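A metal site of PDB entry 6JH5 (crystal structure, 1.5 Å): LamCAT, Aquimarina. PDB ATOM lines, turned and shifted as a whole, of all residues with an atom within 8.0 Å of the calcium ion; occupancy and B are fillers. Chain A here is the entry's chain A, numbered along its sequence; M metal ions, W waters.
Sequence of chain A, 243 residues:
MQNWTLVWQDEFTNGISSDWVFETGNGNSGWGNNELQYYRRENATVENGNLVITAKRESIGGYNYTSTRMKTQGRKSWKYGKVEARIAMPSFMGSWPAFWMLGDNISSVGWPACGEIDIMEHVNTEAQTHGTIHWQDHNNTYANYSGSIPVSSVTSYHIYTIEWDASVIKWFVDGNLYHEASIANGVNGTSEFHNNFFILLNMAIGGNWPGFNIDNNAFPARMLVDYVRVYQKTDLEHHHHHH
The calcium ion is bound by the backbone carbonyl oxygen (O) of Gly 49, the backbone carbonyl oxygen (O) of Glu 11, the backbone carbonyl oxygen (O) of Asp 226, water W2 and the side-chain carboxylate (OD1) of Asp 226.
The side-chain carboxylate (OD1) of Asp 226 lies close to the side-chain amide nitrogen (ND2) of Asn 50 (3.4 Å).
NE of Arg 229 lies within salt-bridge range of OE2 of Glu 11, at 2.8 Å.
OD2 of Asp 226 is in salt-bridge range of NH1 of Arg 86 (2.7 Å).
Three residues have an atom within 4 Å of the calcium ion: Glu 11, Gly 49 and Asp 226.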
ATOM      1  N   ASP A  10      -5.496  -1.140 -16.154  1.00  0.00           N
ATOM      2  CA  ASP A  10      -5.832  -1.666 -14.812  1.00  0.00           C
ATOM      3  C   ASP A  10      -4.669  -2.605 -14.443  1.00  0.00           C
ATOM      4  O   ASP A  10      -4.511  -3.567 -15.100  1.00  0.00           O
ATOM      5  CB  ASP A  10      -7.180  -2.359 -14.677  1.00  0.00           C
ATOM      6  CG  ASP A  10      -7.631  -2.434 -13.229  1.00  0.00           C
ATOM      7  OD1 ASP A  10      -6.780  -2.304 -12.361  1.00  0.00           O
ATOM      8  OD2 ASP A  10      -8.793  -2.612 -12.998  1.00  0.00           O
ATOM      9  N   GLU A  11      -3.873  -2.186 -13.477  1.00  0.00           N
ATOM     10  CA  GLU A  11      -2.722  -2.983 -12.995  1.00  0.00           C
ATOM     11  C   GLU A  11      -3.143  -3.891 -11.845  1.00  0.00           C
ATOM     12  O   GLU A  11      -2.316  -4.620 -11.400  1.00  0.00           O
ATOM     13  CB  GLU A  11      -1.613  -2.044 -12.524  1.00  0.00           C
ATOM     14  CG  GLU A  11      -1.142  -1.113 -13.598  1.00  0.00           C
ATOM     15  CD  GLU A  11      -0.416  -1.784 -14.751  1.00  0.00           C
ATOM     16  OE1 GLU A  11       0.342  -2.707 -14.495  1.00  0.00           O
ATOM     17  OE2 GLU A  11      -0.641  -1.372 -15.853  1.00  0.00           O
ATOM     18  N   PHE A  12      -4.357  -3.718 -11.332  1.00  0.00           N
ATOM     19  CA  PHE A  12      -4.899  -4.572 -10.257  1.00  0.00           C
ATOM     20  C   PHE A  12      -3.967  -4.561  -9.045  1.00  0.00           C
ATOM     21  O   PHE A  12      -3.796  -5.572  -8.439  1.00  0.00           O
ATOM     22  CB  PHE A  12      -5.086  -5.993 -10.785  1.00  0.00           C
ATOM     23  CG  PHE A  12      -5.981  -6.091 -11.989  1.00  0.00           C
ATOM     24  CD1 PHE A  12      -7.323  -5.826 -11.867  1.00  0.00           C
ATOM     25  CD2 PHE A  12      -5.483  -6.465 -13.215  1.00  0.00           C
ATOM     26  CE1 PHE A  12      -8.158  -5.922 -12.966  1.00  0.00           C
ATOM     27  CE2 PHE A  12      -6.317  -6.539 -14.316  1.00  0.00           C
ATOM     28  CZ  PHE A  12      -7.654  -6.277 -14.178  1.00  0.00           C
ATOM     29  N   THR A  13      -3.410  -3.407  -8.732  1.00  0.00           N
ATOM     30  CA  THR A  13      -2.405  -3.432  -7.647  1.00  0.00           C
ATOM     31  C   THR A  13      -3.033  -3.853  -6.306  1.00  0.00           C
ATOM     32  O   THR A  13      -2.476  -4.747  -5.671  1.00  0.00           O
ATOM     33  CB  THR A  13      -1.709  -2.078  -7.601  1.00  0.00           C
ATOM     34  OG1 THR A  13      -1.207  -1.830  -8.901  1.00  0.00           O
ATOM     35  CG2 THR A  13      -0.564  -2.064  -6.612  1.00  0.00           C
ATOM     36  N   ASN A  14      -4.144  -3.236  -5.927  1.00  0.00           N
ATOM     37  CA  ASN A  14      -4.778  -3.613  -4.655  1.00  0.00           C
ATOM     38  C   ASN A  14      -6.216  -4.108  -4.859  1.00  0.00           C
ATOM     39  O   ASN A  14      -6.733  -4.822  -3.997  1.00  0.00           O
ATOM     40  CB  ASN A  14      -4.708  -2.442  -3.681  1.00  0.00           C
ATOM     41  CG  ASN A  14      -3.293  -1.976  -3.415  1.00  0.00           C
ATOM     42  OD1 ASN A  14      -2.907  -0.880  -3.817  1.00  0.00           O
ATOM     43  ND2 ASN A  14      -2.502  -2.826  -2.811  1.00  0.00           N
ATOM     44  N   VAL A  46      -8.583  -9.985  -6.173  1.00  0.00           N
ATOM     45  CA  VAL A  46      -7.216  -9.522  -6.483  1.00  0.00           C
ATOM     46  C   VAL A  46      -6.296 -10.116  -5.424  1.00  0.00           C
ATOM     47  O   VAL A  46      -6.593  -9.990  -4.253  1.00  0.00           O
ATOM     48  CB  VAL A  46      -7.080  -8.001  -6.540  1.00  0.00           C
ATOM     49  CG1 VAL A  46      -5.634  -7.562  -6.522  1.00  0.00           C
ATOM     50  CG2 VAL A  46      -7.778  -7.438  -7.758  1.00  0.00           C
ATOM     51  N   GLU A  47      -5.257 -10.771  -5.876  1.00  0.00           N
ATOM     52  CA  GLU A  47      -4.273 -11.323  -4.939  1.00  0.00           C
ATOM     53  C   GLU A  47      -2.892 -11.003  -5.460  1.00  0.00           C
ATOM     54  O   GLU A  47      -2.638 -11.259  -6.607  1.00  0.00           O
ATOM     55  CB  GLU A  47      -4.249 -12.826  -5.006  1.00  0.00           C
ATOM     56  CG  GLU A  47      -5.495 -13.495  -4.517  1.00  0.00           C
ATOM     57  CD  GLU A  47      -5.319 -14.999  -4.661  1.00  0.00           C
ATOM     58  OE1 GLU A  47      -4.202 -15.440  -4.946  1.00  0.00           O
ATOM     59  OE2 GLU A  47      -6.276 -15.685  -4.557  1.00  0.00           O
ATOM     60  N   ASN A  48      -2.070 -10.456  -4.586  1.00  0.00           N
ATOM     61  CA  ASN A  48      -0.651 -10.297  -4.923  1.00  0.00           C
ATOM     62  C   ASN A  48      -0.507  -9.560  -6.269  1.00  0.00           C
ATOM     63  O   ASN A  48       0.216 -10.043  -7.112  1.00  0.00           O
ATOM     64  CB  ASN A  48       0.029 -11.672  -4.795  1.00  0.00           C
ATOM     65  CG  ASN A  48      -0.053 -12.273  -3.398  1.00  0.00           C
ATOM     66  OD1 ASN A  48      -0.690 -13.296  -3.151  1.00  0.00           O
ATOM     67  ND2 ASN A  48       0.598 -11.625  -2.446  1.00  0.00           N
ATOM     68  N   GLY A  49      -1.262  -8.485  -6.489  1.00  0.00           N
ATOM     69  CA  GLY A  49      -1.136  -7.681  -7.712  1.00  0.00           C
ATOM     70  C   GLY A  49      -1.685  -8.328  -8.995  1.00  0.00           C
ATOM     71  O   GLY A  49      -1.311  -7.889 -10.052  1.00  0.00           O
ATOM     72  N   ASN A  50      -2.550  -9.316  -8.881  1.00  0.00           N
ATOM     73  CA  ASN A  50      -3.129  -9.905 -10.100  1.00  0.00           C
ATOM     74  C   ASN A  50      -4.641 -10.020  -9.923  1.00  0.00           C
ATOM     75  O   ASN A  50      -5.067 -10.305  -8.850  1.00  0.00           O
ATOM     76  CB  ASN A  50      -2.754 -11.367 -10.235  1.00  0.00           C
ATOM     77  CG  ASN A  50      -1.461 -11.671 -10.933  1.00  0.00           C
ATOM     78  OD1 ASN A  50      -1.223 -12.825 -11.284  1.00  0.00           O
ATOM     79  ND2 ASN A  50      -0.600 -10.693 -11.067  1.00  0.00           N
ATOM     80  N   LEU A  51      -5.375  -9.783 -11.004  1.00  0.00           N
ATOM     81  CA  LEU A  51      -6.806 -10.112 -10.993  1.00  0.00           C
ATOM     82  C   LEU A  51      -6.850 -11.648 -11.022  1.00  0.00           C
ATOM     83  O   LEU A  51      -6.067 -12.235 -11.738  1.00  0.00           O
ATOM     84  CB  LEU A  51      -7.480  -9.568 -12.252  1.00  0.00           C
ATOM     85  CG  LEU A  51      -8.831 -10.195 -12.601  1.00  0.00           C
ATOM     86  CD1 LEU A  51      -9.908  -9.761 -11.623  1.00  0.00           C
ATOM     87  CD2 LEU A  51      -9.231  -9.814 -14.000  1.00  0.00           C
ATOM     88  N   ARG A  86      -1.411  -9.273 -19.811  1.00  0.00           N
ATOM     89  CA  ARG A  86      -0.476 -10.358 -19.439  1.00  0.00           C
ATOM     90  C   ARG A  86      -1.295 -11.349 -18.621  1.00  0.00           C
ATOM     91  O   ARG A  86      -1.766 -10.974 -17.599  1.00  0.00           O
ATOM     92  CB  ARG A  86       0.657  -9.769 -18.608  1.00  0.00           C
ATOM     93  CG  ARG A  86       1.696 -10.794 -18.194  1.00  0.00           C
ATOM     94  CD  ARG A  86       3.004 -10.139 -17.778  1.00  0.00           C
ATOM     95  NE  ARG A  86       3.974 -11.158 -17.440  1.00  0.00           N
ATOM     96  CZ  ARG A  86       4.297 -11.534 -16.218  1.00  0.00           C
ATOM     97  NH1 ARG A  86       3.768 -10.980 -15.162  1.00  0.00           N
ATOM     98  NH2 ARG A  86       5.158 -12.513 -16.054  1.00  0.00           N
ATOM     99  N   VAL A 225      -4.677 -12.334 -14.323  1.00  0.00           N
ATOM    100  CA  VAL A 225      -4.361 -11.220 -15.234  1.00  0.00           C
ATOM    101  C   VAL A 225      -3.503 -10.211 -14.451  1.00  0.00           C
ATOM    102  O   VAL A 225      -3.944  -9.716 -13.476  1.00  0.00           O
ATOM    103  CB  VAL A 225      -5.657 -10.590 -15.772  1.00  0.00           C
ATOM    104  CG1 VAL A 225      -5.331  -9.499 -16.777  1.00  0.00           C
ATOM    105  CG2 VAL A 225      -6.543 -11.637 -16.413  1.00  0.00           C
ATOM    106  N   ASP A 226      -2.266 -10.075 -14.879  1.00  0.00           N
ATOM    107  CA  ASP A 226      -1.304  -9.138 -14.253  1.00  0.00           C
ATOM    108  C   ASP A 226      -1.735  -7.710 -14.550  1.00  0.00           C
ATOM    109  O   ASP A 226      -1.688  -6.888 -13.669  1.00  0.00           O
ATOM    110  CB  ASP A 226       0.100  -9.480 -14.752  1.00  0.00           C
ATOM    111  CG  ASP A 226       1.223  -8.814 -13.977  1.00  0.00           C
ATOM    112  OD1 ASP A 226       0.939  -8.250 -12.925  1.00  0.00           O
ATOM    113  OD2 ASP A 226       2.304  -8.853 -14.460  1.00  0.00           O
ATOM    114  N   TYR A 227      -2.099  -7.455 -15.789  1.00  0.00           N
ATOM    115  CA  TYR A 227      -2.588  -6.113 -16.172  1.00  0.00           C
ATOM    116  C   TYR A 227      -3.335  -6.151 -17.495  1.00  0.00           C
ATOM    117  O   TYR A 227      -3.216  -7.086 -18.220  1.00  0.00           O
ATOM    118  CB  TYR A 227      -1.413  -5.154 -16.330  1.00  0.00           C
ATOM    119  CG  TYR A 227      -0.361  -5.599 -17.297  1.00  0.00           C
ATOM    120  CD1 TYR A 227      -0.553  -5.530 -18.656  1.00  0.00           C
ATOM    121  CD2 TYR A 227       0.840  -6.100 -16.839  1.00  0.00           C
ATOM    122  CE1 TYR A 227       0.431  -5.936 -19.544  1.00  0.00           C
ATOM    123  CE2 TYR A 227       1.829  -6.509 -17.712  1.00  0.00           C
ATOM    124  CZ  TYR A 227       1.627  -6.411 -19.068  1.00  0.00           C
ATOM    125  OH  TYR A 227       2.577  -6.791 -19.948  1.00  0.00           O
ATOM    126  N   VAL A 228      -4.098  -5.090 -17.721  1.00  0.00           N
ATOM    127  CA  VAL A 228      -4.725  -4.796 -19.020  1.00  0.00           C
ATOM    128  C   VAL A 228      -4.276  -3.364 -19.356  1.00  0.00           C
ATOM    129  O   VAL A 228      -4.426  -2.534 -18.519  1.00  0.00           O
ATOM    130  CB  VAL A 228      -6.257  -4.879 -18.996  1.00  0.00           C
ATOM    131  CG1 VAL A 228      -6.802  -4.663 -20.391  1.00  0.00           C
ATOM    132  CG2 VAL A 228      -6.739  -6.225 -18.492  1.00  0.00           C
ATOM    133  N   ARG A 229      -3.749  -3.152 -20.548  1.00  0.00           N
ATOM    134  CA  ARG A 229      -3.286  -1.795 -20.903  1.00  0.00           C
ATOM    135  C   ARG A 229      -3.794  -1.419 -22.296  1.00  0.00           C
ATOM    136  O   ARG A 229      -3.833  -2.255 -23.138  1.00  0.00           O
ATOM    137  CB  ARG A 229      -1.760  -1.729 -20.879  1.00  0.00           C
ATOM    138  CG  ARG A 229      -1.181  -1.857 -19.484  1.00  0.00           C
ATOM    139  CD  ARG A 229       0.331  -1.908 -19.460  1.00  0.00           C
ATOM    140  NE  ARG A 229       0.802  -2.190 -18.106  1.00  0.00           N
ATOM    141  CZ  ARG A 229       1.955  -2.756 -17.794  1.00  0.00           C
ATOM    142  NH1 ARG A 229       2.787  -3.129 -18.728  1.00  0.00           N
ATOM    143  NH2 ARG A 229       2.260  -2.945 -16.530  1.00  0.00           N
HETATM  144 CA    CA M   1      -0.390  -6.220 -11.602  1.00  0.00          CA
HETATM  145  O   HOH W   1       0.747  -3.588  -9.825  1.00  0.00           O
HETATM  146  O   HOH W   2       1.153  -4.440 -12.918  1.00  0.00           O
